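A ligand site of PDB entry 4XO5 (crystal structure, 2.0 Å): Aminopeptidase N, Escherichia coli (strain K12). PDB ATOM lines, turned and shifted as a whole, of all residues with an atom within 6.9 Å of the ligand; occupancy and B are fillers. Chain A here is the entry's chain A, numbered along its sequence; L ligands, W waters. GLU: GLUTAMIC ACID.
An oxygen (OE2) of the ligand lies close to the backbone carbonyl oxygen (O) of Ala 634 (2.9 Å). O of the ligand lies within salt-bridge range of NH2 of Arg 682 (2.7 Å). An oxygen (OE1) of the ligand lies within salt-bridge range of the guanidinium group of Arg 637 (2.7 Å).
The side-chain hydroxyl of Thr 641 sits at hydrogen-bond distance from the backbone carbonyl oxygen of Arg 637 (2.8 Å). OG of Ser 714 is in hydrogen-bond range of NH1 of Arg 682, at 2.8 Å. NE of Arg 637 sits at hydrogen-bond distance from O of Pro 616 (2.7 Å). The backbone carbonyl oxygen (O) of Leu 615 sits at hydrogen-bond distance from the guanidinium group (NH2) of Arg 637, 2.9 Å away.
Residues that only touch the ligand: Phe 686, Glu 638, Ala 718 and Thr 641. Hydrophobic or aromatic side chains within 4 Å of the ligand: Ala 634, Phe 686 and Ala 718.
Water W1 lies within hydrogen-bond range of an oxygen (OE2) of the ligand (2.9 Å) and the side-chain carboxylate (OE1) of Glu 638 (3.1 Å).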
ATOM      1  N   LEU A 615      30.925  11.506 -28.885  1.00  0.00           N
ATOM      2  CA  LEU A 615      31.152  11.896 -27.503  1.00  0.00           C
ATOM      3  C   LEU A 615      30.106  11.225 -26.572  1.00  0.00           C
ATOM      4  O   LEU A 615      28.962  11.084 -26.959  1.00  0.00           O
ATOM      5  CB  LEU A 615      31.065  13.414 -27.343  1.00  0.00           C
ATOM      6  CG  LEU A 615      32.140  14.208 -28.128  1.00  0.00           C
ATOM      7  CD1 LEU A 615      31.977  15.660 -27.760  1.00  0.00           C
ATOM      8  CD2 LEU A 615      33.527  13.749 -27.731  1.00  0.00           C
ATOM      9  N   PRO A 616      30.516  10.878 -25.362  1.00  0.00           N
ATOM     10  CA  PRO A 616      29.550  10.398 -24.360  1.00  0.00           C
ATOM     11  C   PRO A 616      28.340  11.318 -24.256  1.00  0.00           C
ATOM     12  O   PRO A 616      28.498  12.548 -24.353  1.00  0.00           O
ATOM     13  CB  PRO A 616      30.357  10.365 -23.090  1.00  0.00           C
ATOM     14  CG  PRO A 616      31.688  10.865 -23.371  1.00  0.00           C
ATOM     15  CD  PRO A 616      31.877  10.955 -24.846  1.00  0.00           C
ATOM     16  N   SER A 617      27.153  10.740 -24.125  1.00  0.00           N
ATOM     17  CA  SER A 617      25.952  11.488 -23.980  1.00  0.00           C
ATOM     18  C   SER A 617      25.970  12.224 -22.619  1.00  0.00           C
ATOM     19  O   SER A 617      26.795  11.913 -21.773  1.00  0.00           O
ATOM     20  CB  SER A 617      24.730  10.582 -23.945  1.00  0.00           C
ATOM     21  OG  SER A 617      24.731   9.789 -22.751  1.00  0.00           O
ATOM     22  N   VAL A 618      25.034  13.147 -22.449  1.00  0.00           N
ATOM     23  CA  VAL A 618      24.940  13.918 -21.218  1.00  0.00           C
ATOM     24  C   VAL A 618      24.620  12.972 -20.065  1.00  0.00           C
ATOM     25  O   VAL A 618      24.973  13.269 -18.907  1.00  0.00           O
ATOM     26  CB  VAL A 618      23.972  15.078 -21.257  1.00  0.00           C
ATOM     27  CG1 VAL A 618      24.396  16.125 -22.296  1.00  0.00           C
ATOM     28  CG2 VAL A 618      22.545  14.630 -21.574  1.00  0.00           C
ATOM     29  N   MET A 621      27.892  11.311 -19.223  1.00  0.00           N
ATOM     30  CA  MET A 621      28.702  12.342 -18.543  1.00  0.00           C
ATOM     31  C   MET A 621      28.319  12.486 -17.087  1.00  0.00           C
ATOM     32  O   MET A 621      29.208  12.571 -16.218  1.00  0.00           O
ATOM     33  CB  MET A 621      28.572  13.686 -19.260  1.00  0.00           C
ATOM     34  CG  MET A 621      29.357  13.714 -20.567  1.00  0.00           C
ATOM     35  SD  MET A 621      28.888  15.109 -21.612  1.00  0.00           S
ATOM     36  CE  MET A 621      30.008  16.360 -20.969  1.00  0.00           C
ATOM     37  N   ILE A 633      27.214  20.269 -17.719  1.00  0.00           N
ATOM     38  CA  ILE A 633      27.522  19.098 -18.527  1.00  0.00           C
ATOM     39  C   ILE A 633      27.096  19.401 -19.969  1.00  0.00           C
ATOM     40  O   ILE A 633      27.865  19.187 -20.901  1.00  0.00           O
ATOM     41  CB  ILE A 633      26.861  17.821 -18.025  1.00  0.00           C
ATOM     42  CG1 ILE A 633      27.550  17.365 -16.749  1.00  0.00           C
ATOM     43  CG2 ILE A 633      26.834  16.733 -19.075  1.00  0.00           C
ATOM     44  CD1 ILE A 633      26.844  16.284 -15.970  1.00  0.00           C
ATOM     45  N   ALA A 634      25.930  19.976 -20.164  1.00  0.00           N
ATOM     46  CA  ALA A 634      25.465  20.242 -21.531  1.00  0.00           C
ATOM     47  C   ALA A 634      26.316  21.263 -22.249  1.00  0.00           C
ATOM     48  O   ALA A 634      26.704  21.079 -23.420  1.00  0.00           O
ATOM     49  CB  ALA A 634      23.982  20.667 -21.536  1.00  0.00           C
ATOM     50  N   GLU A 635      26.721  22.297 -21.530  1.00  0.00           N
ATOM     51  CA  GLU A 635      27.580  23.333 -22.178  1.00  0.00           C
ATOM     52  C   GLU A 635      28.968  22.853 -22.457  1.00  0.00           C
ATOM     53  O   GLU A 635      29.535  23.236 -23.483  1.00  0.00           O
ATOM     54  CB  GLU A 635      27.674  24.593 -21.358  1.00  0.00           C
ATOM     55  CG  GLU A 635      26.354  25.103 -20.873  1.00  0.00           C
ATOM     56  CD  GLU A 635      25.664  26.120 -21.701  1.00  0.00           C
ATOM     57  OE1 GLU A 635      24.802  26.816 -21.077  1.00  0.00           O
ATOM     58  OE2 GLU A 635      25.993  26.208 -22.909  1.00  0.00           O
ATOM     59  N   VAL A 636      29.527  22.023 -21.560  1.00  0.00           N
ATOM     60  CA  VAL A 636      30.834  21.422 -21.808  1.00  0.00           C
ATOM     61  C   VAL A 636      30.807  20.494 -22.987  1.00  0.00           C
ATOM     62  O   VAL A 636      31.747  20.458 -23.775  1.00  0.00           O
ATOM     63  CB  VAL A 636      31.365  20.705 -20.571  1.00  0.00           C
ATOM     64  CG1 VAL A 636      32.565  19.842 -20.850  1.00  0.00           C
ATOM     65  CG2 VAL A 636      31.775  21.783 -19.526  1.00  0.00           C
ATOM     66  N   ARG A 637      29.734  19.700 -23.123  1.00  0.00           N
ATOM     67  CA  ARG A 637      29.639  18.781 -24.259  1.00  0.00           C
ATOM     68  C   ARG A 637      29.646  19.552 -25.541  1.00  0.00           C
ATOM     69  O   ARG A 637      30.378  19.194 -26.474  1.00  0.00           O
ATOM     70  CB  ARG A 637      28.390  17.885 -24.176  1.00  0.00           C
ATOM     71  CG  ARG A 637      28.386  16.753 -25.207  1.00  0.00           C
ATOM     72  CD  ARG A 637      27.176  15.805 -24.970  1.00  0.00           C
ATOM     73  NE  ARG A 637      27.339  14.608 -25.728  1.00  0.00           N
ATOM     74  CZ  ARG A 637      26.918  14.442 -26.978  1.00  0.00           C
ATOM     75  NH1 ARG A 637      26.237  15.378 -27.570  1.00  0.00           N
ATOM     76  NH2 ARG A 637      27.131  13.287 -27.632  1.00  0.00           N
ATOM     77  N   GLU A 638      28.887  20.660 -25.549  1.00  0.00           N
ATOM     78  CA  GLU A 638      28.889  21.558 -26.707  1.00  0.00           C
ATOM     79  C   GLU A 638      30.290  22.183 -26.990  1.00  0.00           C
ATOM     80  O   GLU A 638      30.777  22.222 -28.140  1.00  0.00           O
ATOM     81  CB  GLU A 638      27.815  22.655 -26.603  1.00  0.00           C
ATOM     82  CG  GLU A 638      27.841  23.518 -27.836  1.00  0.00           C
ATOM     83  CD  GLU A 638      26.818  24.680 -27.840  1.00  0.00           C
ATOM     84  OE1 GLU A 638      25.784  24.608 -27.131  1.00  0.00           O
ATOM     85  OE2 GLU A 638      27.071  25.642 -28.645  1.00  0.00           O
ATOM     86  N   ALA A 639      30.898  22.689 -25.923  1.00  0.00           N
ATOM     87  CA  ALA A 639      32.171  23.404 -26.069  1.00  0.00           C
ATOM     88  C   ALA A 639      33.209  22.405 -26.544  1.00  0.00           C
ATOM     89  O   ALA A 639      34.086  22.727 -27.342  1.00  0.00           O
ATOM     90  CB  ALA A 639      32.564  24.072 -24.729  1.00  0.00           C
ATOM     91  N   THR A 641      32.704  19.723 -28.333  1.00  0.00           N
ATOM     92  CA  THR A 641      32.376  19.474 -29.710  1.00  0.00           C
ATOM     93  C   THR A 641      32.956  20.627 -30.605  1.00  0.00           C
ATOM     94  O   THR A 641      33.583  20.365 -31.620  1.00  0.00           O
ATOM     95  CB  THR A 641      30.848  19.303 -29.851  1.00  0.00           C
ATOM     96  OG1 THR A 641      30.491  18.183 -29.042  1.00  0.00           O
ATOM     97  CG2 THR A 641      30.484  19.029 -31.310  1.00  0.00           C
ATOM     98  N   ARG A 682      28.524  15.722 -37.533  1.00  0.00           N
ATOM     99  CA  ARG A 682      28.097  16.311 -36.256  1.00  0.00           C
ATOM    100  C   ARG A 682      29.136  17.395 -35.797  1.00  0.00           C
ATOM    101  O   ARG A 682      28.732  18.471 -35.370  1.00  0.00           O
ATOM    102  CB  ARG A 682      28.015  15.212 -35.170  1.00  0.00           C
ATOM    103  CG  ARG A 682      27.355  15.640 -33.881  1.00  0.00           C
ATOM    104  CD  ARG A 682      25.914  15.957 -34.144  1.00  0.00           C
ATOM    105  NE  ARG A 682      25.190  16.125 -32.892  1.00  0.00           N
ATOM    106  CZ  ARG A 682      23.869  16.066 -32.760  1.00  0.00           C
ATOM    107  NH1 ARG A 682      23.087  15.666 -33.768  1.00  0.00           N
ATOM    108  NH2 ARG A 682      23.360  16.274 -31.574  1.00  0.00           N
ATOM    109  N   PHE A 683      30.415  17.066 -35.834  1.00  0.00           N
ATOM    110  CA  PHE A 683      31.483  18.045 -35.507  1.00  0.00           C
ATOM    111  C   PHE A 683      31.488  19.232 -36.482  1.00  0.00           C
ATOM    112  O   PHE A 683      31.536  20.381 -36.061  1.00  0.00           O
ATOM    113  CB  PHE A 683      32.857  17.361 -35.500  1.00  0.00           C
ATOM    114  CG  PHE A 683      33.085  16.480 -34.299  1.00  0.00           C
ATOM    115  CD1 PHE A 683      33.285  17.046 -33.029  1.00  0.00           C
ATOM    116  CD2 PHE A 683      33.130  15.131 -34.437  1.00  0.00           C
ATOM    117  CE1 PHE A 683      33.520  16.273 -31.953  1.00  0.00           C
ATOM    118  CE2 PHE A 683      33.292  14.305 -33.313  1.00  0.00           C
ATOM    119  CZ  PHE A 683      33.468  14.864 -32.064  1.00  0.00           C
ATOM    120  N   PHE A 686      29.158  22.053 -35.875  1.00  0.00           N
ATOM    121  CA  PHE A 686      29.609  22.920 -34.796  1.00  0.00           C
ATOM    122  C   PHE A 686      30.888  23.706 -35.131  1.00  0.00           C
ATOM    123  O   PHE A 686      31.494  24.298 -34.230  1.00  0.00           O
ATOM    124  CB  PHE A 686      29.819  22.068 -33.541  1.00  0.00           C
ATOM    125  CG  PHE A 686      28.534  21.721 -32.819  1.00  0.00           C
ATOM    126  CD1 PHE A 686      27.982  22.589 -31.905  1.00  0.00           C
ATOM    127  CD2 PHE A 686      27.854  20.548 -33.103  1.00  0.00           C
ATOM    128  CE1 PHE A 686      26.833  22.297 -31.232  1.00  0.00           C
ATOM    129  CE2 PHE A 686      26.667  20.232 -32.416  1.00  0.00           C
ATOM    130  CZ  PHE A 686      26.159  21.095 -31.476  1.00  0.00           C
ATOM    131  N   SER A 714      19.132  16.701 -37.152  1.00  0.00           N
ATOM    132  CA  SER A 714      19.502  16.673 -35.811  1.00  0.00           C
ATOM    133  C   SER A 714      20.731  17.636 -35.582  1.00  0.00           C
ATOM    134  O   SER A 714      20.753  18.370 -34.599  1.00  0.00           O
ATOM    135  CB  SER A 714      19.896  15.245 -35.440  1.00  0.00           C
ATOM    136  OG  SER A 714      20.286  15.303 -34.115  1.00  0.00           O
ATOM    137  N   ALA A 718      20.920  20.846 -33.085  1.00  0.00           N
ATOM    138  CA  ALA A 718      21.892  20.838 -32.012  1.00  0.00           C
ATOM    139  C   ALA A 718      22.836  22.092 -32.081  1.00  0.00           C
ATOM    140  O   ALA A 718      23.200  22.674 -31.064  1.00  0.00           O
ATOM    141  CB  ALA A 718      22.735  19.585 -32.081  1.00  0.00           C
ATOM    142  N   ALA A 719      23.198  22.492 -33.307  1.00  0.00           N
ATOM    143  CA  ALA A 719      24.096  23.622 -33.475  1.00  0.00           C
ATOM    144  C   ALA A 719      23.345  24.900 -33.757  1.00  0.00           C
ATOM    145  O   ALA A 719      23.990  25.903 -33.978  1.00  0.00           O
ATOM    146  CB  ALA A 719      25.080  23.323 -34.608  1.00  0.00           C
ATOM    147  N   PRO A 753      18.708  22.569 -27.828  1.00  0.00           N
ATOM    148  CA  PRO A 753      19.441  23.431 -26.888  1.00  0.00           C
ATOM    149  C   PRO A 753      18.852  24.851 -26.853  1.00  0.00           C
ATOM    150  O   PRO A 753      19.342  25.693 -26.135  1.00  0.00           O
ATOM    151  CB  PRO A 753      20.847  23.458 -27.484  1.00  0.00           C
ATOM    152  CG  PRO A 753      20.630  23.308 -28.983  1.00  0.00           C
ATOM    153  CD  PRO A 753      19.439  22.368 -29.074  1.00  0.00           C
HETATM  154  N   GLU L   1      24.702  18.007 -29.552  1.00  0.00           N
HETATM  155  CA  GLU L   1      26.078  18.333 -29.681  1.00  0.00           C
HETATM  156  C   GLU L   1      26.418  17.109 -30.283  1.00  0.00           C
HETATM  157  O   GLU L   1      25.694  16.176 -30.161  1.00  0.00           O
HETATM  158  CB  GLU L   1      26.785  18.679 -28.375  1.00  0.00           C
HETATM  159  CG  GLU L   1      26.021  19.664 -27.414  1.00  0.00           C
HETATM  160  CD  GLU L   1      25.335  18.961 -26.241  1.00  0.00           C
HETATM  161  OE1 GLU L   1      25.316  17.748 -26.600  1.00  0.00           O
HETATM  162  OE2 GLU L   1      24.898  19.549 -25.054  1.00  0.00           O
HETATM  163  OXT GLU L   1      27.326  16.894 -31.002  1.00  0.00           O
HETATM  164  O   HOH W   1      24.152  22.247 -25.913  1.00  0.00           O
HETATM  165  O   HOH W   2      23.924  21.763 -28.400  1.00  0.00           O
HETATM  166  O   HOH W   3      22.681  19.220 -28.264  1.00  0.00           O
HETATM  167  O   HOH W   4      22.919  16.402 -25.629  1.00  0.00           O
HETATM  168  O   HOH W   5      22.171  18.697 -24.039  1.00  0.00           O
